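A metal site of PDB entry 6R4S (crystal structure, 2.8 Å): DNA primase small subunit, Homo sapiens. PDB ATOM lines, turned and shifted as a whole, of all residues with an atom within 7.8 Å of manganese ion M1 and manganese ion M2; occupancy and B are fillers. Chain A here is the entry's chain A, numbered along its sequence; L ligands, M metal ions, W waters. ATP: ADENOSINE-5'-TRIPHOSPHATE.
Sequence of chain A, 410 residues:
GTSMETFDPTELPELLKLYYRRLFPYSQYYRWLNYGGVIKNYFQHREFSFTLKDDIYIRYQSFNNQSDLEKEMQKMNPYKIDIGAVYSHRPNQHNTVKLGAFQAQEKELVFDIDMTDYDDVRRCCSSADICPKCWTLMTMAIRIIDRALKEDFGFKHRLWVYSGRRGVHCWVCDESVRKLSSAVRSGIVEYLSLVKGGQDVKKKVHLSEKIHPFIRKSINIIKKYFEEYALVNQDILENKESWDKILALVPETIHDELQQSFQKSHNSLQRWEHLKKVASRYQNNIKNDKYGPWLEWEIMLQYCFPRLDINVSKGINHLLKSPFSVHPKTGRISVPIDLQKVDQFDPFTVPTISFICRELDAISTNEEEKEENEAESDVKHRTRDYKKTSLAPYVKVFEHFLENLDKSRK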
ATOM      1  N   PHE A 111      -4.464 -11.443 -11.309  1.00  0.00           N
ATOM      2  CA  PHE A 111      -4.484 -10.742 -10.033  1.00  0.00           C
ATOM      3  C   PHE A 111      -4.215  -9.263 -10.276  1.00  0.00           C
ATOM      4  O   PHE A 111      -3.299  -8.927 -11.030  1.00  0.00           O
ATOM      5  CB  PHE A 111      -3.444 -11.309  -9.061  1.00  0.00           C
ATOM      6  CG  PHE A 111      -3.594 -12.775  -8.800  1.00  0.00           C
ATOM      7  CD1 PHE A 111      -4.521 -13.245  -7.893  1.00  0.00           C
ATOM      8  CD2 PHE A 111      -2.790 -13.686  -9.475  1.00  0.00           C
ATOM      9  CE1 PHE A 111      -4.649 -14.601  -7.660  1.00  0.00           C
ATOM     10  CE2 PHE A 111      -2.918 -15.042  -9.241  1.00  0.00           C
ATOM     11  CZ  PHE A 111      -3.844 -15.496  -8.322  1.00  0.00           C
ATOM     12  N   ASP A 112      -5.020  -8.401  -9.652  1.00  0.00           N
ATOM     13  CA  ASP A 112      -4.885  -6.960  -9.737  1.00  0.00           C
ATOM     14  C   ASP A 112      -4.614  -6.424  -8.335  1.00  0.00           C
ATOM     15  O   ASP A 112      -5.432  -6.632  -7.432  1.00  0.00           O
ATOM     16  CB  ASP A 112      -6.144  -6.320 -10.322  1.00  0.00           C
ATOM     17  CG  ASP A 112      -6.118  -4.808 -10.289  1.00  0.00           C
ATOM     18  OD1 ASP A 112      -5.070  -4.210 -10.600  1.00  0.00           O
ATOM     19  OD2 ASP A 112      -7.167  -4.217  -9.957  1.00  0.00           O
ATOM     20  N   ILE A 113      -3.490  -5.749  -8.141  1.00  0.00           N
ATOM     21  CA  ILE A 113      -3.129  -5.172  -6.850  1.00  0.00           C
ATOM     22  C   ILE A 113      -3.037  -3.670  -7.021  1.00  0.00           C
ATOM     23  O   ILE A 113      -2.215  -3.184  -7.808  1.00  0.00           O
ATOM     24  CB  ILE A 113      -1.806  -5.726  -6.316  1.00  0.00           C
ATOM     25  CG1 ILE A 113      -1.845  -7.248  -6.350  1.00  0.00           C
ATOM     26  CG2 ILE A 113      -1.578  -5.241  -4.894  1.00  0.00           C
ATOM     27  CD1 ILE A 113      -0.564  -7.915  -5.909  1.00  0.00           C
ATOM     28  N   ASP A 114      -3.869  -2.946  -6.270  1.00  0.00           N
ATOM     29  CA  ASP A 114      -3.919  -1.493  -6.268  1.00  0.00           C
ATOM     30  C   ASP A 114      -3.398  -0.983  -4.929  1.00  0.00           C
ATOM     31  O   ASP A 114      -3.817  -1.467  -3.871  1.00  0.00           O
ATOM     32  CB  ASP A 114      -5.357  -0.999  -6.473  1.00  0.00           C
ATOM     33  CG  ASP A 114      -5.988  -1.539  -7.730  1.00  0.00           C
ATOM     34  OD1 ASP A 114      -5.262  -1.735  -8.727  1.00  0.00           O
ATOM     35  OD2 ASP A 114      -7.217  -1.753  -7.717  1.00  0.00           O
ATOM     36  N   MET A 115      -2.502   0.006  -4.987  1.00  0.00           N
ATOM     37  CA  MET A 115      -1.976   0.595  -3.763  1.00  0.00           C
ATOM     38  C   MET A 115      -3.060   1.321  -2.969  1.00  0.00           C
ATOM     39  O   MET A 115      -2.894   1.502  -1.753  1.00  0.00           O
ATOM     40  CB  MET A 115      -0.865   1.589  -4.111  1.00  0.00           C
ATOM     41  CG  MET A 115      -0.001   2.003  -2.933  1.00  0.00           C
ATOM     42  SD  MET A 115       1.274   0.820  -2.488  1.00  0.00           S
ATOM     43  CE  MET A 115       2.371   0.961  -3.903  1.00  0.00           C
ATOM     44  N   ASP A 117      -5.777   0.315  -1.869  1.00  0.00           N
ATOM     45  CA  ASP A 117      -6.302  -0.523  -0.807  1.00  0.00           C
ATOM     46  C   ASP A 117      -5.414  -0.510   0.436  1.00  0.00           C
ATOM     47  O   ASP A 117      -5.771  -1.165   1.426  1.00  0.00           O
ATOM     48  CB  ASP A 117      -6.484  -1.947  -1.333  1.00  0.00           C
ATOM     49  CG  ASP A 117      -7.391  -2.005  -2.565  1.00  0.00           C
ATOM     50  OD1 ASP A 117      -8.286  -1.137  -2.677  1.00  0.00           O
ATOM     51  OD2 ASP A 117      -7.213  -2.905  -3.403  1.00  0.00           O
ATOM     52  N   SER A 163       1.015  -2.154 -13.493  1.00  0.00           N
ATOM     53  CA  SER A 163      -0.288  -1.710 -13.990  1.00  0.00           C
ATOM     54  C   SER A 163      -0.235  -0.315 -14.601  1.00  0.00           C
ATOM     55  O   SER A 163      -1.234   0.113 -15.193  1.00  0.00           O
ATOM     56  CB  SER A 163      -1.327  -1.740 -12.882  1.00  0.00           C
ATOM     57  OG  SER A 163      -1.021  -0.785 -11.881  1.00  0.00           O
ATOM     58  N   GLY A 164       0.875   0.406 -14.462  1.00  0.00           N
ATOM     59  CA  GLY A 164       1.023   1.709 -15.050  1.00  0.00           C
ATOM     60  C   GLY A 164       0.816   2.877 -14.109  1.00  0.00           C
ATOM     61  O   GLY A 164       1.171   4.001 -14.449  1.00  0.00           O
ATOM     62  N   ARG A 165       0.275   2.642 -12.916  1.00  0.00           N
ATOM     63  CA  ARG A 165       0.019   3.742 -11.997  1.00  0.00           C
ATOM     64  C   ARG A 165       0.218   3.330 -10.543  1.00  0.00           C
ATOM     65  O   ARG A 165       1.192   3.734  -9.911  1.00  0.00           O
ATOM     66  CB  ARG A 165      -1.400   4.289 -12.208  1.00  0.00           C
ATOM     67  CG  ARG A 165      -1.691   5.534 -11.417  1.00  0.00           C
ATOM     68  CD  ARG A 165      -2.990   6.177 -11.858  1.00  0.00           C
ATOM     69  NE  ARG A 165      -4.174   5.541 -11.308  1.00  0.00           N
ATOM     70  CZ  ARG A 165      -5.424   5.944 -11.550  1.00  0.00           C
ATOM     71  NH1 ARG A 165      -5.641   6.998 -12.329  1.00  0.00           N
ATOM     72  NH2 ARG A 165      -6.442   5.310 -11.006  1.00  0.00           N
ATOM     73  N   ARG A 166      -0.711   2.529 -10.008  1.00  0.00           N
ATOM     74  CA  ARG A 166      -0.820   2.328  -8.573  1.00  0.00           C
ATOM     75  C   ARG A 166      -0.675   0.879  -8.142  1.00  0.00           C
ATOM     76  O   ARG A 166      -1.130   0.506  -7.060  1.00  0.00           O
ATOM     77  CB  ARG A 166      -2.168   2.881  -8.076  1.00  0.00           C
ATOM     78  CG  ARG A 166      -3.348   2.146  -8.671  1.00  0.00           C
ATOM     79  CD  ARG A 166      -4.663   2.785  -8.268  1.00  0.00           C
ATOM     80  NE  ARG A 166      -5.782   2.109  -8.896  1.00  0.00           N
ATOM     81  CZ  ARG A 166      -7.053   2.401  -8.661  1.00  0.00           C
ATOM     82  NH1 ARG A 166      -8.009   1.729  -9.280  1.00  0.00           N
ATOM     83  NH2 ARG A 166      -7.370   3.360  -7.799  1.00  0.00           N
ATOM     84  N   GLY A 167      -0.072   0.026  -8.962  1.00  0.00           N
ATOM     85  CA  GLY A 167       0.100  -1.352  -8.544  1.00  0.00           C
ATOM     86  C   GLY A 167       0.551  -2.238  -9.673  1.00  0.00           C
ATOM     87  O   GLY A 167       1.139  -1.776 -10.658  1.00  0.00           O
ATOM     88  N   VAL A 168       0.279  -3.534  -9.513  1.00  0.00           N
ATOM     89  CA  VAL A 168       0.777  -4.540 -10.449  1.00  0.00           C
ATOM     90  C   VAL A 168      -0.303  -5.565 -10.773  1.00  0.00           C
ATOM     91  O   VAL A 168      -1.354  -5.637 -10.124  1.00  0.00           O
ATOM     92  CB  VAL A 168       2.051  -5.258  -9.928  1.00  0.00           C
ATOM     93  CG1 VAL A 168       3.167  -4.257  -9.643  1.00  0.00           C
ATOM     94  CG2 VAL A 168       1.734  -6.080  -8.702  1.00  0.00           C
ATOM     95  N   HIS A 169      -0.033  -6.348 -11.801  1.00  0.00           N
ATOM     96  CA  HIS A 169      -0.884  -7.427 -12.261  1.00  0.00           C
ATOM     97  C   HIS A 169      -0.071  -8.698 -12.358  1.00  0.00           C
ATOM     98  O   HIS A 169       1.149  -8.660 -12.535  1.00  0.00           O
ATOM     99  CB  HIS A 169      -1.508  -7.129 -13.619  1.00  0.00           C
ATOM    100  CG  HIS A 169      -2.394  -5.931 -13.615  1.00  0.00           C
ATOM    101  ND1 HIS A 169      -2.794  -5.303 -14.770  1.00  0.00           N
ATOM    102  CD2 HIS A 169      -2.955  -5.242 -12.596  1.00  0.00           C
ATOM    103  CE1 HIS A 169      -3.571  -4.276 -14.469  1.00  0.00           C
ATOM    104  NE2 HIS A 169      -3.682  -4.223 -13.158  1.00  0.00           N
ATOM    105  N   LEU A 308      -5.634  -8.094  -2.224  1.00  0.00           N
ATOM    106  CA  LEU A 308      -5.971  -8.261  -3.629  1.00  0.00           C
ATOM    107  C   LEU A 308      -7.382  -7.744  -3.899  1.00  0.00           C
ATOM    108  O   LEU A 308      -8.290  -7.936  -3.086  1.00  0.00           O
ATOM    109  CB  LEU A 308      -5.891  -9.726  -4.086  1.00  0.00           C
ATOM    110  CG  LEU A 308      -4.523 -10.411  -4.196  1.00  0.00           C
ATOM    111  CD1 LEU A 308      -4.659 -11.785  -4.822  1.00  0.00           C
ATOM    112  CD2 LEU A 308      -3.576  -9.569  -4.976  1.00  0.00           C
ATOM    113  N   ASP A 309      -7.547  -7.093  -5.047  1.00  0.00           N
ATOM    114  CA  ASP A 309      -8.863  -6.791  -5.590  1.00  0.00           C
ATOM    115  C   ASP A 309      -9.532  -8.107  -5.967  1.00  0.00           C
ATOM    116  O   ASP A 309      -9.171  -8.725  -6.972  1.00  0.00           O
ATOM    117  CB  ASP A 309      -8.726  -5.858  -6.788  1.00  0.00           C
ATOM    118  CG  ASP A 309      -9.976  -5.028  -7.035  1.00  0.00           C
ATOM    119  OD1 ASP A 309     -11.088  -5.471  -6.670  1.00  0.00           O
ATOM    120  OD2 ASP A 309      -9.853  -3.917  -7.605  1.00  0.00           O
ATOM    121  N   ILE A 310     -10.494  -8.535  -5.157  1.00  0.00           N
ATOM    122  CA  ILE A 310     -10.939  -9.930  -5.190  1.00  0.00           C
ATOM    123  C   ILE A 310     -11.746 -10.214  -6.457  1.00  0.00           C
ATOM    124  O   ILE A 310     -11.477 -11.188  -7.166  1.00  0.00           O
ATOM    125  CB  ILE A 310     -11.740 -10.255  -3.918  1.00  0.00           C
ATOM    126  CG1 ILE A 310     -10.821 -10.232  -2.691  1.00  0.00           C
ATOM    127  CG2 ILE A 310     -12.425 -11.618  -4.027  1.00  0.00           C
ATOM    128  CD1 ILE A 310     -11.548 -10.285  -1.366  1.00  0.00           C
ATOM    129  N   VAL A 312     -11.657  -9.235  -9.249  1.00  0.00           N
ATOM    130  CA  VAL A 312     -10.898  -9.314 -10.493  1.00  0.00           C
ATOM    131  C   VAL A 312     -10.568 -10.766 -10.820  1.00  0.00           C
ATOM    132  O   VAL A 312     -10.524 -11.145 -12.005  1.00  0.00           O
ATOM    133  CB  VAL A 312      -9.618  -8.468 -10.386  1.00  0.00           C
ATOM    134  CG1 VAL A 312      -8.837  -8.478 -11.703  1.00  0.00           C
ATOM    135  CG2 VAL A 312      -9.955  -7.038  -9.983  1.00  0.00           C
ATOM    136  N   HIS A 318     -13.851 -11.503 -16.829  1.00  0.00           N
ATOM    137  CA  HIS A 318     -13.404 -10.174 -16.425  1.00  0.00           C
ATOM    138  C   HIS A 318     -12.236  -9.741 -17.298  1.00  0.00           C
ATOM    139  O   HIS A 318     -11.337 -10.525 -17.596  1.00  0.00           O
ATOM    140  CB  HIS A 318     -13.002 -10.182 -14.953  1.00  0.00           C
ATOM    141  CG  HIS A 318     -12.964  -8.833 -14.317  1.00  0.00           C
ATOM    142  ND1 HIS A 318     -11.905  -7.962 -14.472  1.00  0.00           N
ATOM    143  CD2 HIS A 318     -13.857  -8.189 -13.522  1.00  0.00           C
ATOM    144  CE1 HIS A 318     -12.142  -6.851 -13.793  1.00  0.00           C
ATOM    145  NE2 HIS A 318     -13.322  -6.975 -13.210  1.00  0.00           N
ATOM    146  N   LEU A 320      -8.862  -7.444 -18.195  1.00  0.00           N
ATOM    147  CA  LEU A 320      -7.705  -6.875 -17.519  1.00  0.00           C
ATOM    148  C   LEU A 320      -6.793  -6.214 -18.534  1.00  0.00           C
ATOM    149  O   LEU A 320      -6.624  -6.714 -19.647  1.00  0.00           O
ATOM    150  CB  LEU A 320      -6.926  -7.938 -16.732  1.00  0.00           C
ATOM    151  CG  LEU A 320      -5.767  -7.407 -15.879  1.00  0.00           C
ATOM    152  CD1 LEU A 320      -6.251  -6.474 -14.773  1.00  0.00           C
ATOM    153  CD2 LEU A 320      -5.002  -8.571 -15.270  1.00  0.00           C
ATOM    154  N   LYS A 321      -6.188  -5.106 -18.129  1.00  0.00           N
ATOM    155  CA  LYS A 321      -5.390  -4.306 -19.047  1.00  0.00           C
ATOM    156  C   LYS A 321      -4.247  -5.146 -19.610  1.00  0.00           C
ATOM    157  O   LYS A 321      -3.542  -5.842 -18.873  1.00  0.00           O
ATOM    158  CB  LYS A 321      -4.836  -3.079 -18.335  1.00  0.00           C
ATOM    159  CG  LYS A 321      -4.202  -2.074 -19.282  1.00  0.00           C
ATOM    160  CD  LYS A 321      -4.063  -0.729 -18.621  1.00  0.00           C
ATOM    161  CE  LYS A 321      -3.021  -0.821 -17.538  1.00  0.00           C
ATOM    162  NZ  LYS A 321      -2.627   0.505 -17.027  1.00  0.00           N
ATOM    163  N   HIS A 327      -1.249   3.237 -19.965  1.00  0.00           N
ATOM    164  CA  HIS A 327      -2.169   3.750 -18.957  1.00  0.00           C
ATOM    165  C   HIS A 327      -2.529   5.182 -19.339  1.00  0.00           C
ATOM    166  O   HIS A 327      -1.670   6.070 -19.235  1.00  0.00           O
ATOM    167  CB  HIS A 327      -1.530   3.711 -17.586  1.00  0.00           C
ATOM    168  CG  HIS A 327      -2.519   3.816 -16.460  1.00  0.00           C
ATOM    169  ND1 HIS A 327      -3.418   4.861 -16.359  1.00  0.00           N
ATOM    170  CD2 HIS A 327      -2.756   3.019 -15.403  1.00  0.00           C
ATOM    171  CE1 HIS A 327      -4.152   4.699 -15.283  1.00  0.00           C
ATOM    172  NE2 HIS A 327      -3.783   3.583 -14.686  1.00  0.00           N
HETATM  173  PG  ATP L   1      -4.331   0.947 -12.062  1.00  0.00           P
HETATM  174  O1G ATP L   1      -4.859   2.314 -11.863  1.00  0.00           O
HETATM  175  O2G ATP L   1      -4.805  -0.059 -10.990  1.00  0.00           O
HETATM  176  O3G ATP L   1      -2.810   0.898 -12.022  1.00  0.00           O
HETATM  177  PB  ATP L   1      -5.446  -1.018 -13.856  1.00  0.00           P
HETATM  178  O1B ATP L   1      -5.206  -1.306 -15.275  1.00  0.00           O
HETATM  179  O2B ATP L   1      -4.929  -2.020 -12.810  1.00  0.00           O
HETATM  180  O3B ATP L   1      -4.819   0.403 -13.477  1.00  0.00           O
HETATM  181  PA  ATP L   1      -7.963  -0.883 -12.312  1.00  0.00           P
HETATM  182  O1A ATP L   1      -8.696   0.390 -12.116  1.00  0.00           O
HETATM  183  O2A ATP L   1      -7.107  -1.345 -11.115  1.00  0.00           O
HETATM  184  O3A ATP L   1      -7.002  -0.803 -13.587  1.00  0.00           O
HETATM  185  O5' ATP L   1      -8.895  -2.129 -12.683  1.00  0.00           O
HETATM  186  C5' ATP L   1      -8.260  -3.282 -13.276  1.00  0.00           C
HETATM  187  C4' ATP L   1      -8.956  -3.746 -14.524  1.00  0.00           C
HETATM  188  O4' ATP L   1     -10.368  -3.522 -14.443  1.00  0.00           O
HETATM  189  C3' ATP L   1      -8.523  -2.990 -15.777  1.00  0.00           C
HETATM  190  O3' ATP L   1      -7.358  -3.553 -16.367  1.00  0.00           O
HETATM  191  C2' ATP L   1      -9.760  -3.115 -16.694  1.00  0.00           C
HETATM  192  O2' ATP L   1      -9.533  -4.085 -17.707  1.00  0.00           O
HETATM  193  C1' ATP L   1     -10.869  -3.579 -15.757  1.00  0.00           C
HETATM  194  N9  ATP L   1     -12.039  -2.716 -15.830  1.00  0.00           N
HETATM  195  C8  ATP L   1     -12.145  -1.473 -15.268  1.00  0.00           C
HETATM  196  N7  ATP L   1     -13.265  -0.850 -15.560  1.00  0.00           N
HETATM  197  C5  ATP L   1     -13.941  -1.756 -16.355  1.00  0.00           C
HETATM  198  C6  ATP L   1     -15.188  -1.684 -17.019  1.00  0.00           C
HETATM  199  N6  ATP L   1     -16.000  -0.634 -16.951  1.00  0.00           N
HETATM  200  N1  ATP L   1     -15.558  -2.745 -17.767  1.00  0.00           N
HETATM  201  C2  ATP L   1     -14.733  -3.800 -17.846  1.00  0.00           C
HETATM  202  N3  ATP L   1     -13.538  -3.975 -17.272  1.00  0.00           N
HETATM  203  C4  ATP L   1     -13.206  -2.909 -16.541  1.00  0.00           C
HETATM  204 MN    MN M   1      -8.545  -2.818  -9.005  1.00  0.00          MN
HETATM  205 MN    MN M   2      -4.944  -2.045 -10.786  1.00  0.00          MN
HETATM  206  O   HOH W   1      -2.758  -2.288 -10.469  1.00  0.00           O
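His 169 touches manganese ion M2. Of the 21 residues printed, 3 come within 4 Å of manganese ion M2.
The side-chain carboxylate (OD1) of Asp 114 lies close to the guanidinium group (NE) of Arg 166, at 3.9 Å. The side-chain carboxylate (OD1) of Asp 112 sits close to a ring nitrogen (NE2) of His 169 (2.9 Å).
Water W1 lies within hydrogen-bond range of OG of Ser 163 (2.7 Å), O of Ile 113 (2.9 Å), N of Val 168 (3.4 Å) and NE2 of His 169 (3.4 Å).
Manganese ion M1 is bound by OD2 of Asp 114 (2.1 Å), OD2 of Asp 112 (2.2 Å) and OD2 of Asp 309 (2.2 Å). Slightly farther from manganese ion M1 lies O2A of the ligand (2.9 Å).
An oxygen (O2G) of the ligand is bound to manganese ion M2 (2.0 Å). Manganese ion M2 is bound by an oxygen (O2B) of the ligand (2.0 Å). OD1 of Asp 114 binds manganese ion M2 (2.1 Å). Manganese ion M2 is bound by the side-chain carboxylate (OD1) of Asp 112, 2.2 Å away. Water W1 is bound to manganese ion M2, at 2.2 Å. An oxygen (O2A) of the ligand binds manganese ion M2 (2.3 Å). Manganese ion M2 has six donor atoms within binding distance.
A ring nitrogen (NE2) of His 169 lies close to an oxygen (O2B) of the ligand (2.6 Å). The side-chain hydroxyl (OG) of Ser 163 sits at hydrogen-bond distance from an oxygen (O3G) of the ligand, at 2.5 Å. An oxygen (O3G) of the ligand is in hydrogen-bond range of the backbone NH of Arg 166 (3.3 Å). The guanidinium group of Arg 166 is in salt-bridge range of an oxygen (O1G) of the ligand, at 3.1 Å. An oxygen (O2') of the ligand sits close to the backbone NH (N) of Leu 320, 3.5 Å away. A ring nitrogen (NE2) of His 327 lies within hydrogen-bond range of an oxygen (O1G) of the ligand, 3.3 Å away. An oxygen (O3') of the ligand is in hydrogen-bond range of the backbone NH (N) of Lys 321, at 2.6 Å. An oxygen (O1B) of the ligand lies within salt-bridge range of the side-chain amino group (NZ) of Lys 321 (3.6 Å). The guanidinium group (NE) of Arg 165 is in salt-bridge range of an oxygen (O1G) of the ligand (3.3 Å).
Of the 21 residues printed, 3 come within 4 Å of manganese ion M1.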
